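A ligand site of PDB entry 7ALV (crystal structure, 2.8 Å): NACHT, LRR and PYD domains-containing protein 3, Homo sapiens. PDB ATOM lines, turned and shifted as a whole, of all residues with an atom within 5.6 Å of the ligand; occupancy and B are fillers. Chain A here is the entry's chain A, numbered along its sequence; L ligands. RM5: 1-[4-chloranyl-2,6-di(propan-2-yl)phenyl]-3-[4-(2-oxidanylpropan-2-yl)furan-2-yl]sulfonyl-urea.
An oxygen (O12) of the ligand sits at hydrogen-bond distance from the guanidinium group (NH1) of Arg 222 (2.8 Å). NH1 of Arg 449 lies within hydrogen-bond range of O16 of the ligand (2.9 Å). N of Ala 99 lies within hydrogen-bond range of N10 of the ligand, 3.0 Å away. O of Ala 99 lies close to N15 of the ligand (3.4 Å).
The guanidinium group of Arg 449 is in salt-bridge range of the side-chain carboxylate of Glu 500, at 2.4 Å. The side-chain carboxylate (OD1) of Asp 533 is in hydrogen-bond range of the side-chain hydroxyl (OH) of Tyr 503 (2.5 Å). The backbone NH of Met 532 lies close to the side-chain hydroxyl of Thr 530 (3.4 Å). N of Glu 500 is in hydrogen-bond range of OG of Ser 497. The side-chain hydroxyl of Thr 395 lies within hydrogen-bond range of the side-chain hydroxyl of Tyr 314 (2.9 Å). The side-chain amide nitrogen (NE2) of Gln 495 lies close to the backbone NH (N) of Ser 497 (3.4 Å).
Residues that only touch the ligand: Ala 98, Pro 223, Met 279, Phe 281, Ile 282, Thr 310, Tyr 314, Thr 395, Ile 445, Phe 446, Ser 497, Leu 499, Glu 500, Tyr 503 and Met 532. Hydrophobic or aromatic side chains that line the ligand: Ala 98, Ala 99, Pro 223, Met 279, Phe 281, Ile 282, Ile 445, Phe 446, Leu 499, Tyr 503 and Met 532. Within 4 Å of the ligand: Ala 98, Ala 99, Arg 222, Pro 223, Met 279, Phe 281, Ile 282, Thr 310, Tyr 314, Thr 395, Ile 445, Phe 446, Arg 449, Ser 497, Leu 499, Glu 500, Tyr 503 and Met 532.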
ATOM      1  N   GLY A  97     -32.093  19.653  24.080  1.00  0.00           N
ATOM      2  CA  GLY A  97     -31.733  20.649  25.075  1.00  0.00           C
ATOM      3  C   GLY A  97     -30.560  21.507  24.664  1.00  0.00           C
ATOM      4  O   GLY A  97     -29.532  20.988  24.231  1.00  0.00           O
ATOM      5  N   ALA A  98     -30.696  22.843  24.785  1.00  0.00           N
ATOM      6  CA  ALA A  98     -29.621  23.766  24.398  1.00  0.00           C
ATOM      7  C   ALA A  98     -28.365  23.539  25.234  1.00  0.00           C
ATOM      8  O   ALA A  98     -28.460  23.020  26.346  1.00  0.00           O
ATOM      9  CB  ALA A  98     -30.095  25.202  24.554  1.00  0.00           C
ATOM     10  N   ALA A  99     -27.188  23.949  24.728  1.00  0.00           N
ATOM     11  CA  ALA A  99     -25.941  23.777  25.487  1.00  0.00           C
ATOM     12  C   ALA A  99     -26.020  24.515  26.825  1.00  0.00           C
ATOM     13  O   ALA A  99     -26.478  25.668  26.860  1.00  0.00           O
ATOM     14  CB  ALA A  99     -24.761  24.297  24.699  1.00  0.00           C
ATOM     15  N   GLY A 100     -25.699  23.833  27.905  1.00  0.00           N
ATOM     16  CA  GLY A 100     -25.783  24.407  29.234  1.00  0.00           C
ATOM     17  C   GLY A 100     -27.146  24.278  29.897  1.00  0.00           C
ATOM     18  O   GLY A 100     -27.321  24.777  31.013  1.00  0.00           O
ATOM     19  N   ARG A 222     -28.159  18.470  21.634  1.00  0.00           N
ATOM     20  CA  ARG A 222     -28.374  19.892  21.391  1.00  0.00           C
ATOM     21  C   ARG A 222     -29.310  19.929  20.189  1.00  0.00           C
ATOM     22  O   ARG A 222     -29.164  19.097  19.278  1.00  0.00           O
ATOM     23  CB  ARG A 222     -27.067  20.579  20.988  1.00  0.00           C
ATOM     24  CG  ARG A 222     -26.109  20.841  22.131  1.00  0.00           C
ATOM     25  CD  ARG A 222     -25.235  22.063  21.880  1.00  0.00           C
ATOM     26  NE  ARG A 222     -24.555  22.078  20.592  1.00  0.00           N
ATOM     27  CZ  ARG A 222     -24.049  23.171  20.006  1.00  0.00           C
ATOM     28  NH1 ARG A 222     -24.177  24.363  20.614  1.00  0.00           N
ATOM     29  NH2 ARG A 222     -23.438  23.103  18.843  1.00  0.00           N
ATOM     30  N   PRO A 223     -30.254  20.895  20.151  1.00  0.00           N
ATOM     31  CA  PRO A 223     -31.227  20.955  19.044  1.00  0.00           C
ATOM     32  C   PRO A 223     -30.629  20.891  17.654  1.00  0.00           C
ATOM     33  O   PRO A 223     -31.228  20.312  16.744  1.00  0.00           O
ATOM     34  CB  PRO A 223     -31.932  22.280  19.290  1.00  0.00           C
ATOM     35  CG  PRO A 223     -31.864  22.465  20.725  1.00  0.00           C
ATOM     36  CD  PRO A 223     -30.541  21.928  21.162  1.00  0.00           C
ATOM     37  N   VAL A 224     -29.442  21.465  17.494  1.00  0.00           N
ATOM     38  CA  VAL A 224     -28.701  21.525  16.240  1.00  0.00           C
ATOM     39  C   VAL A 224     -28.461  20.157  15.643  1.00  0.00           C
ATOM     40  O   VAL A 224     -28.780  19.948  14.468  1.00  0.00           O
ATOM     41  CB  VAL A 224     -27.403  22.359  16.338  1.00  0.00           C
ATOM     42  CG1 VAL A 224     -27.707  23.838  16.191  1.00  0.00           C
ATOM     43  CG2 VAL A 224     -26.661  22.090  17.644  1.00  0.00           C
ATOM     44  N   MET A 279     -31.935  35.183  30.608  1.00  0.00           N
ATOM     45  CA  MET A 279     -30.806  34.316  30.306  1.00  0.00           C
ATOM     46  C   MET A 279     -30.627  33.207  31.363  1.00  0.00           C
ATOM     47  O   MET A 279     -30.052  32.161  31.061  1.00  0.00           O
ATOM     48  CB  MET A 279     -29.549  35.191  30.255  1.00  0.00           C
ATOM     49  CG  MET A 279     -28.523  34.747  29.274  1.00  0.00           C
ATOM     50  SD  MET A 279     -27.329  36.084  29.072  1.00  0.00           S
ATOM     51  CE  MET A 279     -27.923  36.848  27.586  1.00  0.00           C
ATOM     52  N   PHE A 281     -32.747  31.069  32.609  1.00  0.00           N
ATOM     53  CA  PHE A 281     -33.494  29.813  32.526  1.00  0.00           C
ATOM     54  C   PHE A 281     -32.460  28.668  32.256  1.00  0.00           C
ATOM     55  O   PHE A 281     -32.711  27.534  32.649  1.00  0.00           O
ATOM     56  CB  PHE A 281     -34.631  29.844  31.485  1.00  0.00           C
ATOM     57  CG  PHE A 281     -34.219  29.652  30.040  1.00  0.00           C
ATOM     58  CD1 PHE A 281     -33.606  30.669  29.326  1.00  0.00           C
ATOM     59  CD2 PHE A 281     -34.487  28.467  29.386  1.00  0.00           C
ATOM     60  CE1 PHE A 281     -33.233  30.493  28.004  1.00  0.00           C
ATOM     61  CE2 PHE A 281     -34.110  28.286  28.056  1.00  0.00           C
ATOM     62  CZ  PHE A 281     -33.478  29.290  27.386  1.00  0.00           C
ATOM     63  N   ILE A 282     -31.287  29.000  31.651  1.00  0.00           N
ATOM     64  CA  ILE A 282     -30.161  28.113  31.358  1.00  0.00           C
ATOM     65  C   ILE A 282     -29.378  27.902  32.653  1.00  0.00           C
ATOM     66  O   ILE A 282     -28.752  28.829  33.157  1.00  0.00           O
ATOM     67  CB  ILE A 282     -29.269  28.742  30.255  1.00  0.00           C
ATOM     68  CG1 ILE A 282     -30.097  29.074  29.019  1.00  0.00           C
ATOM     69  CG2 ILE A 282     -28.125  27.837  29.881  1.00  0.00           C
ATOM     70  CD1 ILE A 282     -29.635  30.230  28.345  1.00  0.00           C
ATOM     71  N   LEU A 284     -26.526  26.582  33.272  1.00  0.00           N
ATOM     72  CA  LEU A 284     -25.116  26.945  33.167  1.00  0.00           C
ATOM     73  C   LEU A 284     -24.956  28.454  33.405  1.00  0.00           C
ATOM     74  O   LEU A 284     -24.176  28.838  34.273  1.00  0.00           O
ATOM     75  CB  LEU A 284     -24.475  26.519  31.846  1.00  0.00           C
ATOM     76  CG  LEU A 284     -23.018  26.946  31.652  1.00  0.00           C
ATOM     77  CD1 LEU A 284     -22.117  26.419  32.722  1.00  0.00           C
ATOM     78  CD2 LEU A 284     -22.480  26.507  30.307  1.00  0.00           C
ATOM     79  N   VAL A 285     -25.836  29.290  32.797  1.00  0.00           N
ATOM     80  CA  VAL A 285     -25.867  30.737  33.002  1.00  0.00           C
ATOM     81  C   VAL A 285     -26.045  31.037  34.488  1.00  0.00           C
ATOM     82  O   VAL A 285     -25.273  31.819  35.030  1.00  0.00           O
ATOM     83  CB  VAL A 285     -26.937  31.401  32.130  1.00  0.00           C
ATOM     84  CG1 VAL A 285     -27.173  32.846  32.556  1.00  0.00           C
ATOM     85  CG2 VAL A 285     -26.541  31.331  30.682  1.00  0.00           C
ATOM     86  N   THR A 310     -24.617  37.343  26.035  1.00  0.00           N
ATOM     87  CA  THR A 310     -23.950  36.112  26.471  1.00  0.00           C
ATOM     88  C   THR A 310     -22.448  36.330  26.528  1.00  0.00           C
ATOM     89  O   THR A 310     -21.830  35.982  27.528  1.00  0.00           O
ATOM     90  CB  THR A 310     -24.237  34.953  25.521  1.00  0.00           C
ATOM     91  OG1 THR A 310     -25.634  34.784  25.365  1.00  0.00           O
ATOM     92  CG2 THR A 310     -23.611  33.653  25.987  1.00  0.00           C
ATOM     93  N   TYR A 314     -19.863  35.856  29.809  1.00  0.00           N
ATOM     94  CA  TYR A 314     -18.638  35.063  29.749  1.00  0.00           C
ATOM     95  C   TYR A 314     -17.408  35.909  30.046  1.00  0.00           C
ATOM     96  O   TYR A 314     -16.494  35.456  30.732  1.00  0.00           O
ATOM     97  CB  TYR A 314     -18.538  34.364  28.387  1.00  0.00           C
ATOM     98  CG  TYR A 314     -19.314  33.067  28.363  1.00  0.00           C
ATOM     99  CD1 TYR A 314     -20.695  33.058  28.495  1.00  0.00           C
ATOM    100  CD2 TYR A 314     -18.660  31.837  28.264  1.00  0.00           C
ATOM    101  CE1 TYR A 314     -21.411  31.858  28.538  1.00  0.00           C
ATOM    102  CE2 TYR A 314     -19.366  30.644  28.295  1.00  0.00           C
ATOM    103  CZ  TYR A 314     -20.737  30.657  28.433  1.00  0.00           C
ATOM    104  OH  TYR A 314     -21.447  29.482  28.491  1.00  0.00           O
ATOM    105  N   THR A 395     -19.063  25.385  25.697  1.00  0.00           N
ATOM    106  CA  THR A 395     -19.323  26.820  25.421  1.00  0.00           C
ATOM    107  C   THR A 395     -18.068  27.655  25.777  1.00  0.00           C
ATOM    108  O   THR A 395     -17.728  28.605  25.091  1.00  0.00           O
ATOM    109  CB  THR A 395     -20.545  27.300  26.193  1.00  0.00           C
ATOM    110  OG1 THR A 395     -20.426  26.950  27.570  1.00  0.00           O
ATOM    111  CG2 THR A 395     -21.833  26.765  25.630  1.00  0.00           C
ATOM    112  N   ILE A 445     -21.418  27.028  16.524  1.00  0.00           N
ATOM    113  CA  ILE A 445     -22.466  27.944  16.907  1.00  0.00           C
ATOM    114  C   ILE A 445     -21.931  28.992  17.880  1.00  0.00           C
ATOM    115  O   ILE A 445     -22.120  30.182  17.646  1.00  0.00           O
ATOM    116  CB  ILE A 445     -23.711  27.152  17.419  1.00  0.00           C
ATOM    117  CG1 ILE A 445     -24.761  27.005  16.312  1.00  0.00           C
ATOM    118  CG2 ILE A 445     -24.378  27.795  18.626  1.00  0.00           C
ATOM    119  CD1 ILE A 445     -24.442  26.124  15.230  1.00  0.00           C
ATOM    120  N   PHE A 446     -21.229  28.569  18.933  1.00  0.00           N
ATOM    121  CA  PHE A 446     -20.695  29.500  19.923  1.00  0.00           C
ATOM    122  C   PHE A 446     -19.404  30.181  19.501  1.00  0.00           C
ATOM    123  O   PHE A 446     -19.118  31.242  20.019  1.00  0.00           O
ATOM    124  CB  PHE A 446     -20.530  28.867  21.285  1.00  0.00           C
ATOM    125  CG  PHE A 446     -21.795  28.188  21.733  1.00  0.00           C
ATOM    126  CD1 PHE A 446     -22.960  28.912  21.880  1.00  0.00           C
ATOM    127  CD2 PHE A 446     -21.840  26.825  21.925  1.00  0.00           C
ATOM    128  CE1 PHE A 446     -24.135  28.293  22.265  1.00  0.00           C
ATOM    129  CE2 PHE A 446     -23.011  26.202  22.302  1.00  0.00           C
ATOM    130  CZ  PHE A 446     -24.152  26.936  22.470  1.00  0.00           C
ATOM    131  N   ARG A 449     -20.995  32.987  17.216  1.00  0.00           N
ATOM    132  CA  ARG A 449     -21.853  33.788  18.081  1.00  0.00           C
ATOM    133  C   ARG A 449     -21.041  34.566  19.111  1.00  0.00           C
ATOM    134  O   ARG A 449     -21.406  35.685  19.436  1.00  0.00           O
ATOM    135  CB  ARG A 449     -22.871  32.876  18.765  1.00  0.00           C
ATOM    136  CG  ARG A 449     -23.961  33.594  19.484  1.00  0.00           C
ATOM    137  CD  ARG A 449     -24.668  32.631  20.410  1.00  0.00           C
ATOM    138  NE  ARG A 449     -25.573  31.729  19.684  1.00  0.00           N
ATOM    139  CZ  ARG A 449     -26.431  30.915  20.309  1.00  0.00           C
ATOM    140  NH1 ARG A 449     -26.501  30.870  21.622  1.00  0.00           N
ATOM    141  NH2 ARG A 449     -27.227  30.143  19.569  1.00  0.00           N
ATOM    142  N   PHE A 450     -19.903  34.010  19.584  1.00  0.00           N
ATOM    143  CA  PHE A 450     -19.079  34.705  20.552  1.00  0.00           C
ATOM    144  C   PHE A 450     -18.269  35.771  19.920  1.00  0.00           C
ATOM    145  O   PHE A 450     -18.154  36.841  20.504  1.00  0.00           O
ATOM    146  CB  PHE A 450     -18.165  33.764  21.331  1.00  0.00           C
ATOM    147  CG  PHE A 450     -18.791  33.288  22.622  1.00  0.00           C
ATOM    148  CD1 PHE A 450     -19.336  34.186  23.516  1.00  0.00           C
ATOM    149  CD2 PHE A 450     -18.822  31.947  22.938  1.00  0.00           C
ATOM    150  CE1 PHE A 450     -19.900  33.753  24.700  1.00  0.00           C
ATOM    151  CE2 PHE A 450     -19.392  31.513  24.107  1.00  0.00           C
ATOM    152  CZ  PHE A 450     -19.932  32.409  24.979  1.00  0.00           C
ATOM    153  N   GLN A 495     -28.106  25.224   9.473  1.00  0.00           N
ATOM    154  CA  GLN A 495     -27.536  26.370  10.203  1.00  0.00           C
ATOM    155  C   GLN A 495     -26.726  27.308   9.285  1.00  0.00           C
ATOM    156  O   GLN A 495     -26.073  26.856   8.333  1.00  0.00           O
ATOM    157  CB  GLN A 495     -26.693  25.888  11.407  1.00  0.00           C
ATOM    158  CG  GLN A 495     -27.516  25.268  12.543  1.00  0.00           C
ATOM    159  CD  GLN A 495     -28.359  26.253  13.336  1.00  0.00           C
ATOM    160  OE1 GLN A 495     -27.888  26.911  14.269  1.00  0.00           O
ATOM    161  NE2 GLN A 495     -29.643  26.328  13.010  1.00  0.00           N
ATOM    162  N   SER A 497     -29.853  29.168  11.220  1.00  0.00           N
ATOM    163  CA  SER A 497     -31.270  29.451  11.034  1.00  0.00           C
ATOM    164  C   SER A 497     -31.443  30.959  11.175  1.00  0.00           C
ATOM    165  O   SER A 497     -30.554  31.626  11.720  1.00  0.00           O
ATOM    166  CB  SER A 497     -32.077  28.758  12.118  1.00  0.00           C
ATOM    167  OG  SER A 497     -31.665  29.199  13.403  1.00  0.00           O
ATOM    168  N   LEU A 499     -33.230  32.526  13.298  1.00  0.00           N
ATOM    169  CA  LEU A 499     -33.165  32.781  14.742  1.00  0.00           C
ATOM    170  C   LEU A 499     -31.725  32.765  15.198  1.00  0.00           C
ATOM    171  O   LEU A 499     -31.307  33.683  15.898  1.00  0.00           O
ATOM    172  CB  LEU A 499     -33.993  31.763  15.529  1.00  0.00           C
ATOM    173  CG  LEU A 499     -34.098  32.005  17.027  1.00  0.00           C
ATOM    174  CD1 LEU A 499     -35.169  33.014  17.356  1.00  0.00           C
ATOM    175  CD2 LEU A 499     -34.423  30.738  17.753  1.00  0.00           C
ATOM    176  N   GLU A 500     -30.908  31.807  14.722  1.00  0.00           N
ATOM    177  CA  GLU A 500     -29.490  31.767  15.089  1.00  0.00           C
ATOM    178  C   GLU A 500     -28.772  33.031  14.637  1.00  0.00           C
ATOM    179  O   GLU A 500     -27.968  33.563  15.381  1.00  0.00           O
ATOM    180  CB  GLU A 500     -28.794  30.514  14.551  1.00  0.00           C
ATOM    181  CG  GLU A 500     -27.335  30.428  14.943  1.00  0.00           C
ATOM    182  CD  GLU A 500     -27.039  30.528  16.426  1.00  0.00           C
ATOM    183  OE1 GLU A 500     -27.635  29.741  17.195  1.00  0.00           O
ATOM    184  OE2 GLU A 500     -26.223  31.391  16.816  1.00  0.00           O
ATOM    185  N   TYR A 503     -29.514  35.633  17.126  1.00  0.00           N
ATOM    186  CA  TYR A 503     -28.710  35.473  18.326  1.00  0.00           C
ATOM    187  C   TYR A 503     -27.328  36.060  18.101  1.00  0.00           C
ATOM    188  O   TYR A 503     -26.814  36.753  18.975  1.00  0.00           O
ATOM    189  CB  TYR A 503     -28.581  34.003  18.730  1.00  0.00           C
ATOM    190  CG  TYR A 503     -29.675  33.571  19.682  1.00  0.00           C
ATOM    191  CD1 TYR A 503     -29.529  33.753  21.046  1.00  0.00           C
ATOM    192  CD2 TYR A 503     -30.833  32.978  19.226  1.00  0.00           C
ATOM    193  CE1 TYR A 503     -30.520  33.356  21.933  1.00  0.00           C
ATOM    194  CE2 TYR A 503     -31.838  32.591  20.098  1.00  0.00           C
ATOM    195  CZ  TYR A 503     -31.691  32.801  21.447  1.00  0.00           C
ATOM    196  OH  TYR A 503     -32.654  32.420  22.327  1.00  0.00           O
ATOM    197  N   THR A 530     -38.580  30.199  23.394  1.00  0.00           N
ATOM    198  CA  THR A 530     -38.380  30.684  24.741  1.00  0.00           C
ATOM    199  C   THR A 530     -38.491  32.200  24.848  1.00  0.00           C
ATOM    200  O   THR A 530     -38.474  32.874  23.820  1.00  0.00           O
ATOM    201  CB  THR A 530     -37.053  30.147  25.296  1.00  0.00           C
ATOM    202  OG1 THR A 530     -36.801  30.719  26.582  1.00  0.00           O
ATOM    203  CG2 THR A 530     -35.868  30.412  24.376  1.00  0.00           C
ATOM    204  N   MET A 532     -36.164  33.993  25.798  1.00  0.00           N
ATOM    205  CA  MET A 532     -34.844  34.396  25.375  1.00  0.00           C
ATOM    206  C   MET A 532     -34.923  34.638  23.839  1.00  0.00           C
ATOM    207  O   MET A 532     -34.395  35.637  23.358  1.00  0.00           O
ATOM    208  CB  MET A 532     -33.824  33.311  25.718  1.00  0.00           C
ATOM    209  CG  MET A 532     -32.396  33.703  25.439  1.00  0.00           C
ATOM    210  SD  MET A 532     -31.849  35.114  26.439  1.00  0.00           S
ATOM    211  CE  MET A 532     -30.555  35.762  25.396  1.00  0.00           C
ATOM    212  N   ASP A 533     -35.629  33.761  23.094  1.00  0.00           N
ATOM    213  CA  ASP A 533     -35.876  33.916  21.669  1.00  0.00           C
ATOM    214  C   ASP A 533     -36.665  35.195  21.431  1.00  0.00           C
ATOM    215  O   ASP A 533     -36.436  35.870  20.432  1.00  0.00           O
ATOM    216  CB  ASP A 533     -36.682  32.742  21.106  1.00  0.00           C
ATOM    217  CG  ASP A 533     -35.974  31.393  21.081  1.00  0.00           C
ATOM    218  OD1 ASP A 533     -34.761  31.366  21.365  1.00  0.00           O
ATOM    219  OD2 ASP A 533     -36.639  30.370  20.792  1.00  0.00           O
HETATM  220  C1  RM5 L   1     -31.053  26.457  20.417  1.00  0.00           C
HETATM  221  C2  RM5 L   1     -30.607  26.991  19.261  1.00  0.00           C
HETATM  222  C3  RM5 L   1     -29.180  26.670  19.308  1.00  0.00           C
HETATM  223  C13 RM5 L   1     -31.198  29.290  18.436  1.00  0.00           C
HETATM  224  C14 RM5 L   1     -27.509  27.263  22.908  1.00  0.00           C
HETATM  225  C17 RM5 L   1     -27.522  28.914  24.662  1.00  0.00           C
HETATM  226  C18 RM5 L   1     -28.776  29.549  24.477  1.00  0.00           C
HETATM  227  C19 RM5 L   1     -28.956  30.851  24.928  1.00  0.00           C
HETATM  228  C20 RM5 L   1     -27.925  31.497  25.591  1.00  0.00           C
HETATM  229  C21 RM5 L   1     -26.702  30.853  25.829  1.00  0.00           C
HETATM  230  C22 RM5 L   1     -26.484  29.551  25.361  1.00  0.00           C
HETATM  231  C24 RM5 L   1     -29.960  28.855  23.783  1.00  0.00           C
HETATM  232  C25 RM5 L   1     -31.107  28.734  24.806  1.00  0.00           C
HETATM  233  C26 RM5 L   1     -30.444  29.575  22.499  1.00  0.00           C
HETATM  234  C27 RM5 L   1     -25.106  28.925  25.675  1.00  0.00           C
HETATM  235  C28 RM5 L   1     -23.988  29.960  25.348  1.00  0.00           C
HETATM  236  C29 RM5 L   1     -25.016  28.611  27.181  1.00  0.00           C
HETATM  237  C4  RM5 L   1     -29.064  26.009  20.467  1.00  0.00           C
HETATM  238  O5  RM5 L   1     -30.158  25.839  21.201  1.00  0.00           O
HETATM  239  C6  RM5 L   1     -31.364  27.769  18.202  1.00  0.00           C
HETATM  240  O7  RM5 L   1     -30.884  27.421  16.899  1.00  0.00           O
HETATM  241  C8  RM5 L   1     -32.877  27.439  18.191  1.00  0.00           C
HETATM  242  S9  RM5 L   1     -27.583  25.367  21.041  1.00  0.00           S
HETATM  243  N10 RM5 L   1     -27.509  25.968  22.558  1.00  0.00           N
HETATM  244  O11 RM5 L   1     -27.756  23.954  21.204  1.00  0.00           O
HETATM  245  O12 RM5 L   1     -26.517  25.891  20.238  1.00  0.00           O
HETATM  246  N15 RM5 L   1     -27.474  27.569  24.227  1.00  0.00           N
HETATM  247  O16 RM5 L   1     -27.480  28.152  22.070  1.00  0.00           O
HETATM  248 CL1  RM5 L   1     -28.149  33.152  26.132  1.00  0.00          CL
